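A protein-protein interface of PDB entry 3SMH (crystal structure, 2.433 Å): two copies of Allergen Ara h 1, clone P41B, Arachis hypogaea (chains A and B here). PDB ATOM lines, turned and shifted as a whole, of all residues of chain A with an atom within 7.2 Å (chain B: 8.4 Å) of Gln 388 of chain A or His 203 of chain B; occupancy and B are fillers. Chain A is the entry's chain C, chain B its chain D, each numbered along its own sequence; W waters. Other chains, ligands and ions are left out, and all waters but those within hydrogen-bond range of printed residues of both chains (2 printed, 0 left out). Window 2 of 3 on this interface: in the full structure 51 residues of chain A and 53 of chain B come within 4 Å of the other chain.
Hydrophobic or aromatic side chains of chain B within 4 Å of the printed part of chain A: Leu 55, Leu 57, Pro 58, Tyr 104, Val 199, His 203 and Leu 207. Of the 11 printed residues of chain A, 6 touch a printed residue of chain B. Printed residues of chain A that touch a printed residue of chain B: Ile 385, Glu 386, Gln 388, Ala 389, Leu 392 and Ala 393. Among the printed residues, 11 pairs touch across the chains. Among the printed residues, no Asp or Glu carboxylate lies within 4 Å of a Lys or Arg side-chain nitrogen of the other chain.
The side-chain carboxylate (OE1) of Glu 386 of chain A is in hydrogen-bond range of the side-chain hydroxyl (OH) of Tyr 104 of chain B (2.7 Å). ND1 of His 203 of chain B is in hydrogen-bond range of OE1 of Gln 388 of chain A, at 2.9 Å.
Of chain B, only His 203 (2.9 Å) and Leu 207 (3.8 Å) come within 4 Å of Gln 388 of chain A. His 203 of chain B touches just one residue of chain A: Gln 388. Printed residues of chain B within 4 Å of Ala 389 of chain A: Tyr 104. Of the printed residues of chain B, Glu 386 of chain A touches Arg 84 (3.8 Å), Tyr 104 (2.7 Å) and Leu 207 (3.8 Å). Of the printed residues of chain B, Ala 393 of chain A touches Leu 57. Printed residues of chain A within 4 Å of Leu 57 of chain B: Ala 393 (3.9 Å). Of the printed residues of chain B, Leu 392 of chain A touches Leu 55 and Val 199. Ser 200 of chain B touches none of the printed residues of chain A. The nearest printed residue of chain B that does not touch Glu 386 of chain A is Glu 206 of chain B (4.6 Å).
No position is printed for both chains. Of the 11 pairs that touch across the chains among the printed residues, none has its exchanged pair printed and touching as well.
CG of Pro 58 of chain B touches CG2 of Ile 385 of chain A, 3.9 Å away. Tyr 104 of chain B touches Ile 385 of chain A (CE1 to CG2, 3.8 Å). CG of Glu 386 of chain A touches NH1 of Arg 84 of chain B (3.8 Å). Leu 207 of chain B touches Glu 386 of chain A. CB of Gln 388 of chain A touches CD2 of Leu 207 of chain B, at 3.8 Å. Ala 389 of chain A touches Tyr 104 of chain B. CD2 of Leu 55 of chain B touches CD1 of Leu 392 of chain A, 3.7 Å away. CD1 of Leu 392 of chain A touches CG2 of Val 199 of chain B (3.8 Å). CG of Leu 57 of chain B touches CB of Ala 393 of chain A (3.9 Å).
Water W1 lies within hydrogen-bond range of the side-chain carboxylate (OE1) of Glu 386 of chain A (2.6 Å) and the backbone carbonyl oxygen (O) of Leu 207 of chain B (2.9 Å). Water W2 bridges O of Leu 207 of chain B and OE2 of Glu 386 of chain A.
O of Val 197 of chain B lies within hydrogen-bond range of N of Leu 55 of chain B. The backbone carbonyl oxygen (O) of Asn 53 of chain B is in hydrogen-bond range of the backbone NH (N) of Val 199 of chain B, 2.9 Å away. OE1 of Gln 388 of chain A lies close to OD2 of Asp 391 of chain A (3.5 Å). The side-chain hydroxyl (OG) of Ser 200 of chain B lies close to the backbone NH (N) of His 203 of chain B (3.1 Å). The backbone carbonyl oxygen (O) of Ile 385 of chain A is in hydrogen-bond range of the side-chain amino group (NZ) of Lys 390 of chain A (2.7 Å).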
ATOM      1  N   ILE A 385     -10.228   1.960   0.518  1.00  0.00           N
ATOM      2  CA  ILE A 385      -9.242   0.978   0.975  1.00  0.00           C
ATOM      3  C   ILE A 385      -9.992  -0.258   1.474  1.00  0.00           C
ATOM      4  O   ILE A 385     -10.962  -0.111   2.199  1.00  0.00           O
ATOM      5  CB  ILE A 385      -8.373   1.567   2.093  1.00  0.00           C
ATOM      6  CG1 ILE A 385      -7.779   2.919   1.636  1.00  0.00           C
ATOM      7  CG2 ILE A 385      -7.292   0.562   2.518  1.00  0.00           C
ATOM      8  CD1 ILE A 385      -6.950   3.641   2.684  1.00  0.00           C
ATOM      9  N   GLU A 386      -9.576  -1.451   1.042  1.00  0.00           N
ATOM     10  CA  GLU A 386     -10.140  -2.717   1.541  1.00  0.00           C
ATOM     11  C   GLU A 386     -10.128  -2.802   3.066  1.00  0.00           C
ATOM     12  O   GLU A 386      -9.202  -2.323   3.723  1.00  0.00           O
ATOM     13  CB  GLU A 386      -9.359  -3.918   0.991  1.00  0.00           C
ATOM     14  CG  GLU A 386      -9.829  -4.412  -0.350  1.00  0.00           C
ATOM     15  CD  GLU A 386      -8.761  -5.199  -1.086  1.00  0.00           C
ATOM     16  OE1 GLU A 386      -7.583  -4.784  -1.031  1.00  0.00           O
ATOM     17  OE2 GLU A 386      -9.107  -6.221  -1.724  1.00  0.00           O
ATOM     18  N   LYS A 387     -11.144  -3.451   3.621  1.00  0.00           N
ATOM     19  CA  LYS A 387     -11.249  -3.607   5.069  1.00  0.00           C
ATOM     20  C   LYS A 387      -9.972  -4.170   5.690  1.00  0.00           C
ATOM     21  O   LYS A 387      -9.468  -3.633   6.673  1.00  0.00           O
ATOM     22  CB  LYS A 387     -12.454  -4.474   5.422  1.00  0.00           C
ATOM     23  CG  LYS A 387     -12.703  -4.615   6.913  1.00  0.00           C
ATOM     24  CD  LYS A 387     -13.976  -5.400   7.166  1.00  0.00           C
ATOM     25  CE  LYS A 387     -14.193  -5.660   8.642  1.00  0.00           C
ATOM     26  NZ  LYS A 387     -15.571  -6.176   8.902  1.00  0.00           N
ATOM     27  N   GLN A 388      -9.434  -5.231   5.098  1.00  0.00           N
ATOM     28  CA  GLN A 388      -8.234  -5.857   5.645  1.00  0.00           C
ATOM     29  C   GLN A 388      -7.020  -4.927   5.590  1.00  0.00           C
ATOM     30  O   GLN A 388      -6.121  -5.002   6.433  1.00  0.00           O
ATOM     31  CB  GLN A 388      -7.924  -7.181   4.930  1.00  0.00           C
ATOM     32  CG  GLN A 388      -6.821  -7.983   5.599  1.00  0.00           C
ATOM     33  CD  GLN A 388      -7.182  -8.386   7.028  1.00  0.00           C
ATOM     34  OE1 GLN A 388      -6.450  -8.095   7.982  1.00  0.00           O
ATOM     35  NE2 GLN A 388      -8.311  -9.068   7.174  1.00  0.00           N
ATOM     36  N   ALA A 389      -6.995  -4.054   4.590  1.00  0.00           N
ATOM     37  CA  ALA A 389      -5.901  -3.098   4.451  1.00  0.00           C
ATOM     38  C   ALA A 389      -6.020  -1.977   5.482  1.00  0.00           C
ATOM     39  O   ALA A 389      -5.019  -1.528   6.056  1.00  0.00           O
ATOM     40  CB  ALA A 389      -5.864  -2.532   3.043  1.00  0.00           C
ATOM     41  N   LYS A 390      -7.248  -1.527   5.715  1.00  0.00           N
ATOM     42  CA  LYS A 390      -7.513  -0.557   6.774  1.00  0.00           C
ATOM     43  C   LYS A 390      -7.008  -1.110   8.092  1.00  0.00           C
ATOM     44  O   LYS A 390      -6.416  -0.377   8.895  1.00  0.00           O
ATOM     45  CB  LYS A 390      -9.005  -0.315   6.927  1.00  0.00           C
ATOM     46  CG  LYS A 390      -9.681   0.402   5.792  1.00  0.00           C
ATOM     47  CD  LYS A 390     -11.100   0.772   6.206  1.00  0.00           C
ATOM     48  CE  LYS A 390     -11.837   1.564   5.153  1.00  0.00           C
ATOM     49  NZ  LYS A 390     -12.603   0.689   4.228  1.00  0.00           N
ATOM     50  N   ASP A 391      -7.259  -2.405   8.308  1.00  0.00           N
ATOM     51  CA  ASP A 391      -6.926  -3.075   9.570  1.00  0.00           C
ATOM     52  C   ASP A 391      -5.424  -3.141   9.793  1.00  0.00           C
ATOM     53  O   ASP A 391      -4.947  -2.906  10.898  1.00  0.00           O
ATOM     54  CB  ASP A 391      -7.529  -4.481   9.603  1.00  0.00           C
ATOM     55  CG  ASP A 391      -7.236  -5.225  10.901  1.00  0.00           C
ATOM     56  OD1 ASP A 391      -7.865  -4.885  11.935  1.00  0.00           O
ATOM     57  OD2 ASP A 391      -6.392  -6.159  10.866  1.00  0.00           O
ATOM     58  N   LEU A 392      -4.690  -3.435   8.719  1.00  0.00           N
ATOM     59  CA  LEU A 392      -3.234  -3.508   8.747  1.00  0.00           C
ATOM     60  C   LEU A 392      -2.564  -2.138   8.819  1.00  0.00           C
ATOM     61  O   LEU A 392      -1.461  -2.004   9.346  1.00  0.00           O
ATOM     62  CB  LEU A 392      -2.733  -4.273   7.521  1.00  0.00           C
ATOM     63  CG  LEU A 392      -3.093  -5.764   7.515  1.00  0.00           C
ATOM     64  CD1 LEU A 392      -2.852  -6.396   6.151  1.00  0.00           C
ATOM     65  CD2 LEU A 392      -2.309  -6.497   8.595  1.00  0.00           C
ATOM     66  N   ALA A 393      -3.229  -1.122   8.291  1.00  0.00           N
ATOM     67  CA  ALA A 393      -2.617   0.202   8.227  1.00  0.00           C
ATOM     68  C   ALA A 393      -2.874   1.035   9.483  1.00  0.00           C
ATOM     69  O   ALA A 393      -1.955   1.640  10.033  1.00  0.00           O
ATOM     70  CB  ALA A 393      -3.092   0.947   6.986  1.00  0.00           C
ATOM     71  N   GLY A 398     -10.181  -3.061  11.321  1.00  0.00           N
ATOM     72  CA  GLY A 398     -10.919  -2.738  10.113  1.00  0.00           C
ATOM     73  C   GLY A 398     -12.348  -2.315  10.421  1.00  0.00           C
ATOM     74  O   GLY A 398     -12.868  -1.344   9.856  1.00  0.00           O
ATOM     75  N   GLU A 402     -13.886   1.323   9.742  1.00  0.00           N
ATOM     76  CA  GLU A 402     -15.045   1.452   8.855  1.00  0.00           C
ATOM     77  C   GLU A 402     -16.262   2.071   9.548  1.00  0.00           C
ATOM     78  O   GLU A 402     -17.068   2.741   8.901  1.00  0.00           O
ATOM     79  CB  GLU A 402     -15.399   0.122   8.178  1.00  0.00           C
ATOM     80  CG  GLU A 402     -14.277  -0.393   7.267  1.00  0.00           C
ATOM     81  CD  GLU A 402     -14.753  -1.325   6.165  1.00  0.00           C
ATOM     82  OE1 GLU A 402     -14.000  -1.501   5.179  1.00  0.00           O
ATOM     83  OE2 GLU A 402     -15.866  -1.879   6.272  1.00  0.00           O
ATOM     84  N   ASN B  53       4.509 -12.700   1.745  1.00  0.00           N
ATOM     85  CA  ASN B  53       3.400 -12.341   2.635  1.00  0.00           C
ATOM     86  C   ASN B  53       3.610 -10.995   3.336  1.00  0.00           C
ATOM     87  O   ASN B  53       3.445 -10.865   4.553  1.00  0.00           O
ATOM     88  CB  ASN B  53       3.108 -13.446   3.652  1.00  0.00           C
ATOM     89  CG  ASN B  53       2.876 -14.789   2.995  1.00  0.00           C
ATOM     90  OD1 ASN B  53       3.517 -15.778   3.349  1.00  0.00           O
ATOM     91  ND2 ASN B  53       1.978 -14.829   2.019  1.00  0.00           N
ATOM     92  N   LEU B  55       3.089  -6.556   2.951  1.00  0.00           N
ATOM     93  CA  LEU B  55       2.254  -5.536   2.317  1.00  0.00           C
ATOM     94  C   LEU B  55       2.788  -4.104   2.432  1.00  0.00           C
ATOM     95  O   LEU B  55       3.026  -3.605   3.530  1.00  0.00           O
ATOM     96  CB  LEU B  55       0.846  -5.582   2.877  1.00  0.00           C
ATOM     97  CG  LEU B  55      -0.067  -4.413   2.497  1.00  0.00           C
ATOM     98  CD1 LEU B  55      -0.504  -4.498   1.050  1.00  0.00           C
ATOM     99  CD2 LEU B  55      -1.279  -4.385   3.412  1.00  0.00           C
ATOM    100  N   LEU B  57       1.976  -0.521   2.665  1.00  0.00           N
ATOM    101  CA  LEU B  57       0.761   0.121   3.170  1.00  0.00           C
ATOM    102  C   LEU B  57       0.208   1.178   2.219  1.00  0.00           C
ATOM    103  O   LEU B  57       0.953   1.763   1.457  1.00  0.00           O
ATOM    104  CB  LEU B  57       1.016   0.727   4.555  1.00  0.00           C
ATOM    105  CG  LEU B  57       0.510  -0.077   5.773  1.00  0.00           C
ATOM    106  CD1 LEU B  57       0.224  -1.523   5.445  1.00  0.00           C
ATOM    107  CD2 LEU B  57       1.449   0.008   6.973  1.00  0.00           C
ATOM    108  N   PRO B  58      -1.111   1.399   2.259  1.00  0.00           N
ATOM    109  CA  PRO B  58      -1.790   2.368   1.400  1.00  0.00           C
ATOM    110  C   PRO B  58      -1.146   3.739   1.471  1.00  0.00           C
ATOM    111  O   PRO B  58      -0.733   4.147   2.547  1.00  0.00           O
ATOM    112  CB  PRO B  58      -3.193   2.429   2.002  1.00  0.00           C
ATOM    113  CG  PRO B  58      -3.406   1.080   2.550  1.00  0.00           C
ATOM    114  CD  PRO B  58      -2.064   0.640   3.086  1.00  0.00           C
ATOM    115  N   ARG B  84     -12.221   1.143  -6.578  1.00  0.00           N
ATOM    116  CA  ARG B  84     -11.037   0.401  -6.197  1.00  0.00           C
ATOM    117  C   ARG B  84     -10.917  -0.788  -7.144  1.00  0.00           C
ATOM    118  O   ARG B  84     -11.919  -1.411  -7.492  1.00  0.00           O
ATOM    119  CB  ARG B  84     -11.186  -0.092  -4.750  1.00  0.00           C
ATOM    120  CG  ARG B  84     -10.069  -1.012  -4.295  1.00  0.00           C
ATOM    121  CD  ARG B  84     -10.598  -2.132  -3.405  1.00  0.00           C
ATOM    122  NE  ARG B  84     -11.500  -1.592  -2.393  1.00  0.00           N
ATOM    123  CZ  ARG B  84     -12.585  -2.207  -1.930  1.00  0.00           C
ATOM    124  NH1 ARG B  84     -12.922  -3.403  -2.374  1.00  0.00           N
ATOM    125  NH2 ARG B  84     -13.339  -1.613  -1.025  1.00  0.00           N
ATOM    126  N   TYR B 104      -1.701   0.159  -2.834  1.00  0.00           N
ATOM    127  CA  TYR B 104      -0.875  -0.647  -1.965  1.00  0.00           C
ATOM    128  C   TYR B 104      -0.492  -1.924  -2.675  1.00  0.00           C
ATOM    129  O   TYR B 104      -1.157  -2.320  -3.628  1.00  0.00           O
ATOM    130  CB  TYR B 104      -1.549  -0.928  -0.605  1.00  0.00           C
ATOM    131  CG  TYR B 104      -3.032  -1.242  -0.663  1.00  0.00           C
ATOM    132  CD1 TYR B 104      -3.980  -0.235  -0.571  1.00  0.00           C
ATOM    133  CD2 TYR B 104      -3.480  -2.545  -0.771  1.00  0.00           C
ATOM    134  CE1 TYR B 104      -5.331  -0.523  -0.609  1.00  0.00           C
ATOM    135  CE2 TYR B 104      -4.835  -2.839  -0.810  1.00  0.00           C
ATOM    136  CZ  TYR B 104      -5.753  -1.824  -0.730  1.00  0.00           C
ATOM    137  OH  TYR B 104      -7.097  -2.114  -0.775  1.00  0.00           O
ATOM    138  N   LEU B 106       0.820  -5.950  -2.323  1.00  0.00           N
ATOM    139  CA  LEU B 106       0.902  -7.191  -1.569  1.00  0.00           C
ATOM    140  C   LEU B 106       1.836  -8.174  -2.286  1.00  0.00           C
ATOM    141  O   LEU B 106       1.656  -8.470  -3.472  1.00  0.00           O
ATOM    142  CB  LEU B 106      -0.494  -7.804  -1.484  1.00  0.00           C
ATOM    143  CG  LEU B 106      -0.873  -8.875  -0.452  1.00  0.00           C
ATOM    144  CD1 LEU B 106      -1.337 -10.138  -1.127  1.00  0.00           C
ATOM    145  CD2 LEU B 106       0.228  -9.178   0.560  1.00  0.00           C
ATOM    146  N   VAL B 197       4.577  -4.099   6.062  1.00  0.00           N
ATOM    147  CA  VAL B 197       4.231  -4.922   7.208  1.00  0.00           C
ATOM    148  C   VAL B 197       4.043  -6.382   6.833  1.00  0.00           C
ATOM    149  O   VAL B 197       3.759  -6.694   5.674  1.00  0.00           O
ATOM    150  CB  VAL B 197       2.947  -4.397   7.924  1.00  0.00           C
ATOM    151  CG1 VAL B 197       3.133  -2.962   8.361  1.00  0.00           C
ATOM    152  CG2 VAL B 197       1.713  -4.512   7.031  1.00  0.00           C
ATOM    153  N   LYS B 198       4.207  -7.262   7.826  1.00  0.00           N
ATOM    154  CA  LYS B 198       3.935  -8.689   7.667  1.00  0.00           C
ATOM    155  C   LYS B 198       2.437  -8.939   7.652  1.00  0.00           C
ATOM    156  O   LYS B 198       1.678  -8.287   8.363  1.00  0.00           O
ATOM    157  CB  LYS B 198       4.576  -9.514   8.791  1.00  0.00           C
ATOM    158  CG  LYS B 198       5.953 -10.072   8.471  1.00  0.00           C
ATOM    159  CD  LYS B 198       5.925 -11.032   7.275  1.00  0.00           C
ATOM    160  CE  LYS B 198       5.037 -12.226   7.543  1.00  0.00           C
ATOM    161  NZ  LYS B 198       5.095 -13.200   6.427  1.00  0.00           N
ATOM    162  N   VAL B 199       2.015  -9.889   6.839  1.00  0.00           N
ATOM    163  CA  VAL B 199       0.608 -10.201   6.701  1.00  0.00           C
ATOM    164  C   VAL B 199       0.391 -11.708   6.895  1.00  0.00           C
ATOM    165  O   VAL B 199       1.130 -12.532   6.331  1.00  0.00           O
ATOM    166  CB  VAL B 199       0.102  -9.765   5.304  1.00  0.00           C
ATOM    167  CG1 VAL B 199      -1.329 -10.154   5.100  1.00  0.00           C
ATOM    168  CG2 VAL B 199       0.261  -8.271   5.134  1.00  0.00           C
ATOM    169  N   SER B 200      -0.612 -12.070   7.694  1.00  0.00           N
ATOM    170  CA  SER B 200      -0.928 -13.483   7.909  1.00  0.00           C
ATOM    171  C   SER B 200      -1.492 -14.114   6.646  1.00  0.00           C
ATOM    172  O   SER B 200      -2.024 -13.416   5.780  1.00  0.00           O
ATOM    173  CB  SER B 200      -1.928 -13.660   9.051  1.00  0.00           C
ATOM    174  OG  SER B 200      -3.223 -13.246   8.661  1.00  0.00           O
ATOM    175  N   LYS B 201      -1.374 -15.436   6.556  1.00  0.00           N
ATOM    176  CA  LYS B 201      -1.874 -16.195   5.411  1.00  0.00           C
ATOM    177  C   LYS B 201      -3.356 -15.894   5.190  1.00  0.00           C
ATOM    178  O   LYS B 201      -3.830 -15.772   4.063  1.00  0.00           O
ATOM    179  CB  LYS B 201      -1.697 -17.699   5.665  1.00  0.00           C
ATOM    180  CG  LYS B 201      -2.002 -18.596   4.474  1.00  0.00           C
ATOM    181  CD  LYS B 201      -0.793 -18.714   3.543  1.00  0.00           C
ATOM    182  CE  LYS B 201      -1.149 -19.530   2.310  1.00  0.00           C
ATOM    183  NZ  LYS B 201       0.047 -20.126   1.648  1.00  0.00           N
ATOM    184  N   GLU B 202      -4.087 -15.783   6.289  1.00  0.00           N
ATOM    185  CA  GLU B 202      -5.507 -15.522   6.218  1.00  0.00           C
ATOM    186  C   GLU B 202      -5.778 -14.119   5.672  1.00  0.00           C
ATOM    187  O   GLU B 202      -6.700 -13.901   4.886  1.00  0.00           O
ATOM    188  CB  GLU B 202      -6.118 -15.681   7.608  1.00  0.00           C
ATOM    189  CG  GLU B 202      -7.617 -15.538   7.644  1.00  0.00           C
ATOM    190  CD  GLU B 202      -8.146 -15.495   9.055  1.00  0.00           C
ATOM    191  OE1 GLU B 202      -7.321 -15.499   9.993  1.00  0.00           O
ATOM    192  OE2 GLU B 202      -9.381 -15.454   9.227  1.00  0.00           O
ATOM    193  N   HIS B 203      -4.972 -13.162   6.108  1.00  0.00           N
ATOM    194  CA  HIS B 203      -5.067 -11.799   5.598  1.00  0.00           C
ATOM    195  C   HIS B 203      -4.700 -11.758   4.111  1.00  0.00           C
ATOM    196  O   HIS B 203      -5.357 -11.097   3.316  1.00  0.00           O
ATOM    197  CB  HIS B 203      -4.147 -10.872   6.391  1.00  0.00           C
ATOM    198  CG  HIS B 203      -4.562 -10.671   7.816  1.00  0.00           C
ATOM    199  ND1 HIS B 203      -5.841 -10.932   8.265  1.00  0.00           N
ATOM    200  CD2 HIS B 203      -3.869 -10.226   8.893  1.00  0.00           C
ATOM    201  CE1 HIS B 203      -5.918 -10.661   9.554  1.00  0.00           C
ATOM    202  NE2 HIS B 203      -4.736 -10.230   9.959  1.00  0.00           N
ATOM    203  N   VAL B 204      -3.654 -12.485   3.745  1.00  0.00           N
ATOM    204  CA  VAL B 204      -3.212 -12.554   2.369  1.00  0.00           C
ATOM    205  C   VAL B 204      -4.347 -13.031   1.470  1.00  0.00           C
ATOM    206  O   VAL B 204      -4.636 -12.432   0.433  1.00  0.00           O
ATOM    207  CB  VAL B 204      -1.973 -13.462   2.227  1.00  0.00           C
ATOM    208  CG1 VAL B 204      -1.632 -13.681   0.765  1.00  0.00           C
ATOM    209  CG2 VAL B 204      -0.789 -12.848   2.972  1.00  0.00           C
ATOM    210  N   GLU B 205      -5.013 -14.098   1.884  1.00  0.00           N
ATOM    211  CA  GLU B 205      -6.078 -14.689   1.080  1.00  0.00           C
ATOM    212  C   GLU B 205      -7.275 -13.756   0.979  1.00  0.00           C
ATOM    213  O   GLU B 205      -8.013 -13.761  -0.007  1.00  0.00           O
ATOM    214  CB  GLU B 205      -6.496 -16.036   1.663  1.00  0.00           C
ATOM    215  CG  GLU B 205      -5.381 -17.074   1.629  1.00  0.00           C
ATOM    216  CD  GLU B 205      -5.670 -18.270   2.523  1.00  0.00           C
ATOM    217  OE1 GLU B 205      -6.522 -18.147   3.439  1.00  0.00           O
ATOM    218  OE2 GLU B 205      -5.042 -19.333   2.306  1.00  0.00           O
ATOM    219  N   GLU B 206      -7.464 -12.952   2.012  1.00  0.00           N
ATOM    220  CA  GLU B 206      -8.492 -11.925   2.004  1.00  0.00           C
ATOM    221  C   GLU B 206      -8.193 -10.822   0.959  1.00  0.00           C
ATOM    222  O   GLU B 206      -9.072 -10.375   0.228  1.00  0.00           O
ATOM    223  CB  GLU B 206      -8.585 -11.306   3.394  1.00  0.00           C
ATOM    224  CG  GLU B 206      -9.835 -10.498   3.646  1.00  0.00           C
ATOM    225  CD  GLU B 206     -11.090 -11.349   3.658  1.00  0.00           C
ATOM    226  OE1 GLU B 206     -12.191 -10.802   3.484  1.00  0.00           O
ATOM    227  OE2 GLU B 206     -10.992 -12.569   3.844  1.00  0.00           O
ATOM    228  N   LEU B 207      -6.937 -10.396   0.893  1.00  0.00           N
ATOM    229  CA  LEU B 207      -6.512  -9.352  -0.033  1.00  0.00           C
ATOM    230  C   LEU B 207      -6.454  -9.786  -1.505  1.00  0.00           C
ATOM    231  O   LEU B 207      -6.503  -8.939  -2.393  1.00  0.00           O
ATOM    232  CB  LEU B 207      -5.159  -8.782   0.402  1.00  0.00           C
ATOM    233  CG  LEU B 207      -5.170  -8.090   1.765  1.00  0.00           C
ATOM    234  CD1 LEU B 207      -3.771  -7.896   2.311  1.00  0.00           C
ATOM    235  CD2 LEU B 207      -5.919  -6.757   1.703  1.00  0.00           C
ATOM    236  N   THR B 208      -6.365 -11.090  -1.761  1.00  0.00           N
ATOM    237  CA  THR B 208      -6.269 -11.588  -3.131  1.00  0.00           C
ATOM    238  C   THR B 208      -7.598 -12.105  -3.667  1.00  0.00           C
ATOM    239  O   THR B 208      -7.703 -12.456  -4.838  1.00  0.00           O
ATOM    240  CB  THR B 208      -5.235 -12.721  -3.257  1.00  0.00           C
ATOM    241  OG1 THR B 208      -5.697 -13.863  -2.530  1.00  0.00           O
ATOM    242  CG2 THR B 208      -3.884 -12.287  -2.715  1.00  0.00           C
ATOM    243  N   LYS B 209      -8.613 -12.155  -2.816  1.00  0.00           N
ATOM    244  CA  LYS B 209      -9.866 -12.804  -3.193  1.00  0.00           C
ATOM    245  C   LYS B 209     -10.576 -12.196  -4.399  1.00  0.00           C
ATOM    246  O   LYS B 209     -11.181 -12.912  -5.169  1.00  0.00           O
ATOM    247  CB  LYS B 209     -10.820 -12.904  -2.004  1.00  0.00           C
ATOM    248  CG  LYS B 209     -11.283 -11.577  -1.448  1.00  0.00           C
ATOM    249  CD  LYS B 209     -12.253 -11.772  -0.301  1.00  0.00           C
ATOM    250  CE  LYS B 209     -12.725 -10.435   0.274  1.00  0.00           C
ATOM    251  NZ  LYS B 209     -13.851 -10.600   1.244  1.00  0.00           N
HETATM  252  O   HOH W   1      -5.663  -6.189  -2.166  1.00  0.00           O
HETATM  253  O   HOH W   2      -9.192  -8.728  -3.627  1.00  0.00           O
